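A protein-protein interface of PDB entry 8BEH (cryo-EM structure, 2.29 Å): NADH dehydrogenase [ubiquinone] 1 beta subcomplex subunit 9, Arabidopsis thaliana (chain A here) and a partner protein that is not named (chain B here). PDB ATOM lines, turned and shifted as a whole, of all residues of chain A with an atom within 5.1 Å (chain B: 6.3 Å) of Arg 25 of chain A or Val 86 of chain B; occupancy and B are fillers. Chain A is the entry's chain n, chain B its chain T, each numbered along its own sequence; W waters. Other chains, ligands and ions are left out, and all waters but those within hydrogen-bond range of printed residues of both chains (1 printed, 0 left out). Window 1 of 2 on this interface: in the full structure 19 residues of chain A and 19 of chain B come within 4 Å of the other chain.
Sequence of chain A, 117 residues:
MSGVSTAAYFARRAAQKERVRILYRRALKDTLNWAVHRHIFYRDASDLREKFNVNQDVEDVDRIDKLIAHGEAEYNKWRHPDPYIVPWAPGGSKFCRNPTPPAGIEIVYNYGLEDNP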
ATOM      1  N   VAL A  20      29.105  20.092  14.886  1.00  0.00           N
ATOM      2  CA  VAL A  20      27.727  19.678  14.536  1.00  0.00           C
ATOM      3  C   VAL A  20      27.297  20.325  13.197  1.00  0.00           C
ATOM      4  O   VAL A  20      26.884  19.577  12.347  1.00  0.00           O
ATOM      5  CB  VAL A  20      26.710  19.856  15.678  1.00  0.00           C
ATOM      6  CG1 VAL A  20      25.298  19.465  15.285  1.00  0.00           C
ATOM      7  CG2 VAL A  20      27.153  19.143  16.938  1.00  0.00           C
ATOM      8  N   ARG A  21      27.519  21.623  13.012  1.00  0.00           N
ATOM      9  CA  ARG A  21      27.155  22.343  11.759  1.00  0.00           C
ATOM     10  C   ARG A  21      27.891  21.780  10.536  1.00  0.00           C
ATOM     11  O   ARG A  21      27.302  21.737   9.475  1.00  0.00           O
ATOM     12  CB  ARG A  21      27.308  23.850  11.950  1.00  0.00           C
ATOM     13  CG  ARG A  21      26.244  24.479  12.835  1.00  0.00           C
ATOM     14  CD  ARG A  21      26.244  25.986  12.719  1.00  0.00           C
ATOM     15  NE  ARG A  21      27.593  26.491  12.798  1.00  0.00           N
ATOM     16  CZ  ARG A  21      28.201  26.888  13.903  1.00  0.00           C
ATOM     17  NH1 ARG A  21      27.556  26.893  15.054  1.00  0.00           N
ATOM     18  NH2 ARG A  21      29.455  27.281  13.843  1.00  0.00           N
ATOM     19  N   ILE A  22      29.138  21.372  10.690  1.00  0.00           N
ATOM     20  CA  ILE A  22      29.879  20.803   9.570  1.00  0.00           C
ATOM     21  C   ILE A  22      29.450  19.360   9.313  1.00  0.00           C
ATOM     22  O   ILE A  22      29.325  18.934   8.155  1.00  0.00           O
ATOM     23  CB  ILE A  22      31.392  20.936   9.832  1.00  0.00           C
ATOM     24  CG1 ILE A  22      31.790  22.414   9.737  1.00  0.00           C
ATOM     25  CG2 ILE A  22      32.205  20.063   8.882  1.00  0.00           C
ATOM     26  CD1 ILE A  22      33.267  22.670   9.694  1.00  0.00           C
ATOM     27  N   LEU A  23      29.180  18.614  10.378  1.00  0.00           N
ATOM     28  CA  LEU A  23      28.677  17.226  10.244  1.00  0.00           C
ATOM     29  C   LEU A  23      27.345  17.264   9.479  1.00  0.00           C
ATOM     30  O   LEU A  23      27.192  16.469   8.520  1.00  0.00           O
ATOM     31  CB  LEU A  23      28.511  16.546  11.604  1.00  0.00           C
ATOM     32  CG  LEU A  23      27.832  15.177  11.586  1.00  0.00           C
ATOM     33  CD1 LEU A  23      28.681  14.143  10.873  1.00  0.00           C
ATOM     34  CD2 LEU A  23      27.477  14.706  12.981  1.00  0.00           C
ATOM     35  N   TYR A  24      26.449  18.142   9.877  1.00  0.00           N
ATOM     36  CA  TYR A  24      25.148  18.219   9.225  1.00  0.00           C
ATOM     37  C   TYR A  24      25.289  18.587   7.754  1.00  0.00           C
ATOM     38  O   TYR A  24      24.614  18.007   6.897  1.00  0.00           O
ATOM     39  CB  TYR A  24      24.253  19.227   9.940  1.00  0.00           C
ATOM     40  CG  TYR A  24      22.893  19.360   9.307  1.00  0.00           C
ATOM     41  CD1 TYR A  24      22.126  18.240   9.024  1.00  0.00           C
ATOM     42  CD2 TYR A  24      22.388  20.602   8.958  1.00  0.00           C
ATOM     43  CE1 TYR A  24      20.891  18.354   8.435  1.00  0.00           C
ATOM     44  CE2 TYR A  24      21.148  20.725   8.367  1.00  0.00           C
ATOM     45  CZ  TYR A  24      20.406  19.597   8.107  1.00  0.00           C
ATOM     46  OH  TYR A  24      19.174  19.710   7.516  1.00  0.00           O
ATOM     47  N   ARG A  25      26.143  19.543   7.422  1.00  0.00           N
ATOM     48  CA  ARG A  25      26.373  19.945   6.032  1.00  0.00           C
ATOM     49  C   ARG A  25      26.838  18.753   5.153  1.00  0.00           C
ATOM     50  O   ARG A  25      26.352  18.631   4.044  1.00  0.00           O
ATOM     51  CB  ARG A  25      27.340  21.135   5.975  1.00  0.00           C
ATOM     52  CG  ARG A  25      28.116  21.271   4.679  1.00  0.00           C
ATOM     53  CD  ARG A  25      28.611  22.681   4.471  1.00  0.00           C
ATOM     54  NE  ARG A  25      29.353  22.839   3.240  1.00  0.00           N
ATOM     55  CZ  ARG A  25      28.897  23.448   2.156  1.00  0.00           C
ATOM     56  NH1 ARG A  25      27.687  23.972   2.136  1.00  0.00           N
ATOM     57  NH2 ARG A  25      29.660  23.533   1.093  1.00  0.00           N
ATOM     58  N   ARG A  26      27.741  17.949   5.663  1.00  0.00           N
ATOM     59  CA  ARG A  26      28.333  16.839   4.910  1.00  0.00           C
ATOM     60  C   ARG A  26      27.301  15.711   4.784  1.00  0.00           C
ATOM     61  O   ARG A  26      27.242  15.184   3.721  1.00  0.00           O
ATOM     62  CB  ARG A  26      29.694  16.458   5.518  1.00  0.00           C
ATOM     63  CG  ARG A  26      30.777  17.519   5.499  1.00  0.00           C
ATOM     64  CD  ARG A  26      32.120  16.815   5.537  1.00  0.00           C
ATOM     65  NE  ARG A  26      32.765  16.619   6.818  1.00  0.00           N
ATOM     66  CZ  ARG A  26      33.771  17.350   7.305  1.00  0.00           C
ATOM     67  NH1 ARG A  26      34.290  18.346   6.613  1.00  0.00           N
ATOM     68  NH2 ARG A  26      34.261  17.076   8.495  1.00  0.00           N
ATOM     69  N   ALA A  27      26.540  15.438   5.835  1.00  0.00           N
ATOM     70  CA  ALA A  27      25.473  14.401   5.821  1.00  0.00           C
ATOM     71  C   ALA A  27      24.425  14.797   4.786  1.00  0.00           C
ATOM     72  O   ALA A  27      24.111  13.956   3.954  1.00  0.00           O
ATOM     73  CB  ALA A  27      24.892  14.155   7.215  1.00  0.00           C
ATOM     74  N   LEU A  28      24.091  16.083   4.718  1.00  0.00           N
ATOM     75  CA  LEU A  28      23.053  16.582   3.794  1.00  0.00           C
ATOM     76  C   LEU A  28      23.522  16.459   2.352  1.00  0.00           C
ATOM     77  O   LEU A  28      22.753  15.981   1.545  1.00  0.00           O
ATOM     78  CB  LEU A  28      22.660  17.997   4.224  1.00  0.00           C
ATOM     79  CG  LEU A  28      21.393  18.610   3.651  1.00  0.00           C
ATOM     80  CD1 LEU A  28      20.195  17.718   3.903  1.00  0.00           C
ATOM     81  CD2 LEU A  28      21.184  19.977   4.273  1.00  0.00           C
ATOM     82  N   LYS A  29      24.784  16.753   2.100  1.00  0.00           N
ATOM     83  CA  LYS A  29      25.341  16.711   0.731  1.00  0.00           C
ATOM     84  C   LYS A  29      25.420  15.256   0.255  1.00  0.00           C
ATOM     85  O   LYS A  29      25.086  15.003  -0.895  1.00  0.00           O
ATOM     86  CB  LYS A  29      26.586  17.613   0.673  1.00  0.00           C
ATOM     87  CG  LYS A  29      26.264  18.990   0.110  1.00  0.00           C
ATOM     88  CD  LYS A  29      27.441  19.861  -0.215  1.00  0.00           C
ATOM     89  CE  LYS A  29      27.951  20.578   1.010  1.00  0.00           C
ATOM     90  NZ  LYS A  29      26.829  21.015   1.874  1.00  0.00           N
ATOM     91  N   PHE B  71      21.113  35.775  10.061  1.00  0.00           N
ATOM     92  CA  PHE B  71      19.990  34.768  10.054  1.00  0.00           C
ATOM     93  C   PHE B  71      19.490  34.391  11.458  1.00  0.00           C
ATOM     94  O   PHE B  71      18.315  34.045  11.550  1.00  0.00           O
ATOM     95  CB  PHE B  71      20.261  33.533   9.191  1.00  0.00           C
ATOM     96  CG  PHE B  71      20.901  33.723   7.845  1.00  0.00           C
ATOM     97  CD1 PHE B  71      20.409  34.641   6.933  1.00  0.00           C
ATOM     98  CD2 PHE B  71      21.965  32.923   7.465  1.00  0.00           C
ATOM     99  CE1 PHE B  71      20.996  34.777   5.688  1.00  0.00           C
ATOM    100  CE2 PHE B  71      22.548  33.060   6.215  1.00  0.00           C
ATOM    101  CZ  PHE B  71      22.059  33.991   5.331  1.00  0.00           C
ATOM    102  N   ASP B  81      19.247  25.586   9.994  1.00  0.00           N
ATOM    103  CA  ASP B  81      18.580  26.298   8.911  1.00  0.00           C
ATOM    104  C   ASP B  81      19.579  27.102   8.099  1.00  0.00           C
ATOM    105  O   ASP B  81      19.476  27.178   6.870  1.00  0.00           O
ATOM    106  CB  ASP B  81      17.493  27.210   9.475  1.00  0.00           C
ATOM    107  CG  ASP B  81      16.678  26.539  10.557  1.00  0.00           C
ATOM    108  OD1 ASP B  81      16.542  25.301  10.512  1.00  0.00           O
ATOM    109  OD2 ASP B  81      16.169  27.247  11.447  1.00  0.00           O
ATOM    110  N   THR B  82      20.581  27.649   8.770  1.00  0.00           N
ATOM    111  CA  THR B  82      21.612  28.453   8.082  1.00  0.00           C
ATOM    112  C   THR B  82      22.375  27.499   7.159  1.00  0.00           C
ATOM    113  O   THR B  82      22.590  27.856   6.039  1.00  0.00           O
ATOM    114  CB  THR B  82      22.485  29.227   9.097  1.00  0.00           C
ATOM    115  OG1 THR B  82      21.589  30.072   9.816  1.00  0.00           O
ATOM    116  CG2 THR B  82      23.609  30.003   8.455  1.00  0.00           C
ATOM    117  N   VAL B  83      22.700  26.320   7.650  1.00  0.00           N
ATOM    118  CA  VAL B  83      23.411  25.345   6.826  1.00  0.00           C
ATOM    119  C   VAL B  83      22.596  25.000   5.585  1.00  0.00           C
ATOM    120  O   VAL B  83      23.132  24.914   4.472  1.00  0.00           O
ATOM    121  CB  VAL B  83      23.744  24.089   7.655  1.00  0.00           C
ATOM    122  CG1 VAL B  83      24.539  23.110   6.830  1.00  0.00           C
ATOM    123  CG2 VAL B  83      24.512  24.466   8.903  1.00  0.00           C
ATOM    124  N   GLU B  84      21.288  24.800   5.758  1.00  0.00           N
ATOM    125  CA  GLU B  84      20.427  24.536   4.607  1.00  0.00           C
ATOM    126  C   GLU B  84      20.425  25.703   3.622  1.00  0.00           C
ATOM    127  O   GLU B  84      20.487  25.494   2.405  1.00  0.00           O
ATOM    128  CB  GLU B  84      19.005  24.222   5.071  1.00  0.00           C
ATOM    129  CG  GLU B  84      18.865  22.875   5.758  1.00  0.00           C
ATOM    130  CD  GLU B  84      17.740  22.851   6.767  1.00  0.00           C
ATOM    131  OE1 GLU B  84      16.878  23.749   6.717  1.00  0.00           O
ATOM    132  OE2 GLU B  84      17.709  21.928   7.606  1.00  0.00           O
ATOM    133  N   ILE B  85      20.349  26.937   4.126  1.00  0.00           N
ATOM    134  CA  ILE B  85      20.324  28.102   3.244  1.00  0.00           C
ATOM    135  C   ILE B  85      21.647  28.238   2.494  1.00  0.00           C
ATOM    136  O   ILE B  85      21.674  28.601   1.311  1.00  0.00           O
ATOM    137  CB  ILE B  85      19.984  29.379   4.040  1.00  0.00           C
ATOM    138  CG1 ILE B  85      18.482  29.464   4.316  1.00  0.00           C
ATOM    139  CG2 ILE B  85      20.430  30.626   3.292  1.00  0.00           C
ATOM    140  CD1 ILE B  85      18.133  29.927   5.713  1.00  0.00           C
ATOM    141  N   VAL B  86      22.762  27.949   3.165  1.00  0.00           N
ATOM    142  CA  VAL B  86      24.059  28.000   2.497  1.00  0.00           C
ATOM    143  C   VAL B  86      24.140  26.939   1.407  1.00  0.00           C
ATOM    144  O   VAL B  86      24.646  27.200   0.311  1.00  0.00           O
ATOM    145  CB  VAL B  86      25.199  27.866   3.524  1.00  0.00           C
ATOM    146  CG1 VAL B  86      26.535  27.660   2.824  1.00  0.00           C
ATOM    147  CG2 VAL B  86      25.251  29.097   4.411  1.00  0.00           C
ATOM    148  N   MET B  87      23.653  25.711   1.674  1.00  0.00           N
ATOM    149  CA  MET B  87      23.573  24.648   0.631  1.00  0.00           C
ATOM    150  C   MET B  87      22.687  25.118  -0.544  1.00  0.00           C
ATOM    151  O   MET B  87      23.056  24.868  -1.657  1.00  0.00           O
ATOM    152  CB  MET B  87      23.105  23.287   1.169  1.00  0.00           C
ATOM    153  CG  MET B  87      23.043  22.183   0.111  1.00  0.00           C
ATOM    154  SD  MET B  87      22.677  20.478   0.649  1.00  0.00           S
ATOM    155  CE  MET B  87      22.547  19.636  -0.927  1.00  0.00           C
ATOM    156  N   ALA B  88      21.611  25.836  -0.259  1.00  0.00           N
ATOM    157  CA  ALA B  88      20.750  26.321  -1.334  1.00  0.00           C
ATOM    158  C   ALA B  88      21.451  27.385  -2.174  1.00  0.00           C
ATOM    159  O   ALA B  88      21.307  27.407  -3.399  1.00  0.00           O
ATOM    160  CB  ALA B  88      19.445  26.862  -0.760  1.00  0.00           C
ATOM    161  N   ILE B  89      22.209  28.275  -1.532  1.00  0.00           N
ATOM    162  CA  ILE B  89      23.002  29.262  -2.269  1.00  0.00           C
ATOM    163  C   ILE B  89      24.053  28.563  -3.126  1.00  0.00           C
ATOM    164  O   ILE B  89      24.294  28.937  -4.286  1.00  0.00           O
ATOM    165  CB  ILE B  89      23.637  30.267  -1.288  1.00  0.00           C
ATOM    166  CG1 ILE B  89      22.578  31.220  -0.736  1.00  0.00           C
ATOM    167  CG2 ILE B  89      24.760  31.051  -1.954  1.00  0.00           C
ATOM    168  CD1 ILE B  89      22.944  31.839   0.601  1.00  0.00           C
ATOM    169  N   GLU B  90      24.695  27.538  -2.558  1.00  0.00           N
ATOM    170  CA  GLU B  90      25.652  26.714  -3.290  1.00  0.00           C
ATOM    171  C   GLU B  90      25.036  26.167  -4.570  1.00  0.00           C
ATOM    172  O   GLU B  90      25.623  26.267  -5.651  1.00  0.00           O
ATOM    173  CB  GLU B  90      26.115  25.558  -2.401  1.00  0.00           C
ATOM    174  CG  GLU B  90      27.194  25.883  -1.393  1.00  0.00           C
ATOM    175  CD  GLU B  90      28.571  25.830  -2.001  1.00  0.00           C
ATOM    176  OE1 GLU B  90      28.865  26.691  -2.850  1.00  0.00           O
ATOM    177  OE2 GLU B  90      29.359  24.935  -1.633  1.00  0.00           O
ATOM    178  N   GLU B  91      23.781  25.684  -4.556  1.00  0.00           N
ATOM    179  CA  GLU B  91      23.149  25.056  -5.730  1.00  0.00           C
ATOM    180  C   GLU B  91      22.749  26.189  -6.652  1.00  0.00           C
ATOM    181  O   GLU B  91      22.849  26.044  -7.847  1.00  0.00           O
ATOM    182  CB  GLU B  91      21.922  24.195  -5.381  1.00  0.00           C
ATOM    183  CG  GLU B  91      22.233  22.845  -4.780  1.00  0.00           C
ATOM    184  CD  GLU B  91      21.077  21.861  -4.894  1.00  0.00           C
ATOM    185  OE1 GLU B  91      21.153  20.776  -4.295  1.00  0.00           O
ATOM    186  OE2 GLU B  91      20.103  22.185  -5.602  1.00  0.00           O
ATOM    187  N   LEU B  95      28.410  26.392  -6.877  1.00  0.00           N
ATOM    188  CA  LEU B  95      29.713  26.531  -6.248  1.00  0.00           C
ATOM    189  C   LEU B  95      29.933  25.381  -5.279  1.00  0.00           C
ATOM    190  O   LEU B  95      28.992  24.715  -4.844  1.00  0.00           O
ATOM    191  CB  LEU B  95      29.860  27.870  -5.514  1.00  0.00           C
ATOM    192  CG  LEU B  95      29.375  29.126  -6.232  1.00  0.00           C
ATOM    193  CD1 LEU B  95      29.164  30.266  -5.245  1.00  0.00           C
ATOM    194  CD2 LEU B  95      30.319  29.520  -7.348  1.00  0.00           C
ATOM    195  N   GLU B  96      31.198  25.140  -4.957  1.00  0.00           N
ATOM    196  CA  GLU B  96      31.581  24.155  -3.949  1.00  0.00           C
ATOM    197  C   GLU B  96      32.400  24.894  -2.897  1.00  0.00           C
ATOM    198  O   GLU B  96      33.622  25.004  -3.018  1.00  0.00           O
ATOM    199  CB  GLU B  96      32.357  22.994  -4.562  1.00  0.00           C
ATOM    200  CG  GLU B  96      32.520  21.804  -3.631  1.00  0.00           C
ATOM    201  CD  GLU B  96      32.488  20.467  -4.360  1.00  0.00           C
ATOM    202  OE1 GLU B  96      31.621  20.284  -5.233  1.00  0.00           O
ATOM    203  OE2 GLU B  96      33.322  19.594  -4.051  1.00  0.00           O
ATOM    204  N   ILE B  97      31.724  25.412  -1.883  1.00  0.00           N
ATOM    205  CA  ILE B  97      32.401  26.139  -0.808  1.00  0.00           C
ATOM    206  C   ILE B  97      33.070  25.132   0.124  1.00  0.00           C
ATOM    207  O   ILE B  97      32.440  24.130   0.494  1.00  0.00           O
ATOM    208  CB  ILE B  97      31.414  27.018  -0.051  1.00  0.00           C
ATOM    209  CG1 ILE B  97      30.848  28.086  -0.980  1.00  0.00           C
ATOM    210  CG2 ILE B  97      32.094  27.682   1.139  1.00  0.00           C
ATOM    211  CD1 ILE B  97      29.604  28.760  -0.467  1.00  0.00           C
ATOM    212  N   PRO B  98      34.330  25.340   0.496  1.00  0.00           N
ATOM    213  CA  PRO B  98      34.950  24.483   1.512  1.00  0.00           C
ATOM    214  C   PRO B  98      34.224  24.588   2.846  1.00  0.00           C
ATOM    215  O   PRO B  98      33.714  25.647   3.220  1.00  0.00           O
ATOM    216  CB  PRO B  98      36.379  25.023   1.601  1.00  0.00           C
ATOM    217  CG  PRO B  98      36.614  25.652   0.275  1.00  0.00           C
ATOM    218  CD  PRO B  98      35.306  26.245  -0.130  1.00  0.00           C
ATOM    219  N   ASP B  99      34.195  23.465   3.567  1.00  0.00           N
ATOM    220  CA  ASP B  99      33.360  23.347   4.760  1.00  0.00           C
ATOM    221  C   ASP B  99      33.735  24.363   5.832  1.00  0.00           C
ATOM    222  O   ASP B  99      32.860  24.833   6.568  1.00  0.00           O
ATOM    223  CB  ASP B  99      33.451  21.930   5.322  1.00  0.00           C
ATOM    224  CG  ASP B  99      32.707  20.917   4.476  1.00  0.00           C
ATOM    225  OD1 ASP B  99      31.997  21.325   3.535  1.00  0.00           O
ATOM    226  OD2 ASP B  99      32.842  19.704   4.746  1.00  0.00           O
ATOM    227  N   ALA B 102      32.088  27.577   4.607  1.00  0.00           N
ATOM    228  CA  ALA B 102      30.631  27.513   4.628  1.00  0.00           C
ATOM    229  C   ALA B 102      30.088  27.754   6.032  1.00  0.00           C
ATOM    230  O   ALA B 102      29.055  28.410   6.201  1.00  0.00           O
ATOM    231  CB  ALA B 102      30.151  26.168   4.084  1.00  0.00           C
ATOM    232  N   ASP B 103      30.772  27.231   7.052  1.00  0.00           N
ATOM    233  CA  ASP B 103      30.325  27.437   8.423  1.00  0.00           C
ATOM    234  C   ASP B 103      30.469  28.885   8.875  1.00  0.00           C
ATOM    235  O   ASP B 103      29.791  29.292   9.822  1.00  0.00           O
ATOM    236  CB  ASP B 103      31.087  26.513   9.371  1.00  0.00           C
ATOM    237  CG  ASP B 103      30.275  26.147  10.598  1.00  0.00           C
ATOM    238  OD1 ASP B 103      29.138  26.642  10.729  1.00  0.00           O
ATOM    239  OD2 ASP B 103      30.772  25.368  11.433  1.00  0.00           O
ATOM    240  N   ILE B 105      29.788  31.659   6.809  1.00  0.00           N
ATOM    241  CA  ILE B 105      28.637  32.421   6.229  1.00  0.00           C
ATOM    242  C   ILE B 105      27.400  32.324   7.144  1.00  0.00           C
ATOM    243  O   ILE B 105      26.829  31.251   7.194  1.00  0.00           O
ATOM    244  CB  ILE B 105      28.350  31.989   4.781  1.00  0.00           C
ATOM    245  CG1 ILE B 105      29.595  32.140   3.907  1.00  0.00           C
ATOM    246  CG2 ILE B 105      27.171  32.777   4.247  1.00  0.00           C
ATOM    247  CD1 ILE B 105      29.633  31.252   2.708  1.00  0.00           C
ATOM    248  N   ASP B 106      26.972  33.414   7.783  1.00  0.00           N
ATOM    249  CA  ASP B 106      25.875  33.370   8.788  1.00  0.00           C
ATOM    250  C   ASP B 106      24.901  34.507   8.528  1.00  0.00           C
ATOM    251  O   ASP B 106      23.999  34.722   9.318  1.00  0.00           O
ATOM    252  CB  ASP B 106      26.376  33.533  10.221  1.00  0.00           C
ATOM    253  CG  ASP B 106      26.939  34.909  10.502  1.00  0.00           C
ATOM    254  OD1 ASP B 106      27.468  35.535   9.561  1.00  0.00           O
ATOM    255  OD2 ASP B 106      26.845  35.346  11.658  1.00  0.00           O
ATOM    256  N   ALA B 111      27.159  35.960   2.615  1.00  0.00           N
ATOM    257  CA  ALA B 111      26.918  35.129   1.440  1.00  0.00           C
ATOM    258  C   ALA B 111      27.035  35.943   0.157  1.00  0.00           C
ATOM    259  O   ALA B 111      27.617  35.478  -0.831  1.00  0.00           O
ATOM    260  CB  ALA B 111      25.543  34.472   1.541  1.00  0.00           C
HETATM  261  O   HOH W   1      25.862  24.559   3.974  1.00  0.00           O
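The guanidinium group (NE) of Arg 25 of chain A lies within salt-bridge range of the side-chain carboxylate (OD1) of Asp 99 of chain B, at 3.1 Å.
The guanidinium group (NH1) of Arg 26 of chain A lies within salt-bridge range of the side-chain carboxylate (OD2) of Asp 99 of chain B, at 2.7 Å.
OE2 of Glu 84 of chain B is in hydrogen-bond range of OH of Tyr 24 of chain A (2.7 Å).
NH2 of Arg 25 of chain A lies within hydrogen-bond range of O of Ile 97 of chain B.
The guanidinium group (NE) of Arg 21 of chain A is in salt-bridge range of the side-chain carboxylate (OD1) of Asp 103 of chain B, at 2.6 Å.
The guanidinium group (NH2) of Arg 25 of chain A is in salt-bridge range of the side-chain carboxylate (OE2) of Glu 90 of chain B (3.1 Å).
The backbone carbonyl oxygen (O) of Arg 25 of chain A sits close to the side-chain amino group (NZ) of Lys 29 of chain A (3.3 Å).
The backbone NH (N) of Ile 97 of chain B is in hydrogen-bond range of the side-chain carboxylate (OE2) of Glu 90 of chain B, at 2.4 Å.
The backbone carbonyl oxygen of Glu 90 of chain B sits at hydrogen-bond distance from the backbone NH of Leu 95 of chain B, 3.0 Å away.
Among the printed residues, pairs that only touch across the chains: Arg 21 of chain A with Val 83 of chain B, Ile 22 of chain A with Asp 99 of chain B, Ile 22 of chain A with Asp 103 of chain B, Tyr 24 of chain A with Val 83 of chain B, Arg 25 of chain A with Val 83 of chain B, Arg 25 of chain A with Val 86 of chain B, Arg 25 of chain A with Ala 102 of chain B, Leu 28 of chain A with Glu 84 of chain B, Leu 28 of chain A with Met 87 of chain B and Lys 29 of chain A with Met 87 of chain B.
Of the printed residues of chain B, Arg 21 of chain A touches Val 83 (3.9 Å) and Asp 103 (2.6 Å).
Printed residues of chain B within 4 Å of Tyr 24 of chain A: Val 83 (3.9 Å) and Glu 84 (2.7 Å).
Of the printed residues of chain B, Arg 25 of chain A touches Val 83 (3.5 Å), Val 86 (3.9 Å), Glu 90 (3.1 Å), Ile 97 (2.9 Å), Asp 99 (3.1 Å) and Ala 102 (3.5 Å).
Printed residues of chain B within 4 Å of Arg 26 of chain A: Asp 99.
Printed residues of chain A within 4 Å of Val 83 of chain B: Arg 21, Tyr 24 and Arg 25.
Of chain A, only Arg 25 comes within 4 Å of Val 86 of chain B.
Glu 96 of chain B touches none of the printed residues of chain A.
Printed residues of chain A within 4 Å of Ile 97 of chain B: Arg 25.
Ile 105 of chain B touches none of the printed residues of chain A.
Of the 10 printed residues of chain A, 7 touch a printed residue of chain B.
Hydrophobic or aromatic side chains of chain A that line the printed part of chain B: Ile 22, Tyr 24 and Leu 28.
Among the printed residues, 16 pairs touch across the chains.
Water W1 lies within hydrogen-bond range of NH1 of Arg 25 of chain A, O of Val 83 of chain B and N of Met 87 of chain B.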
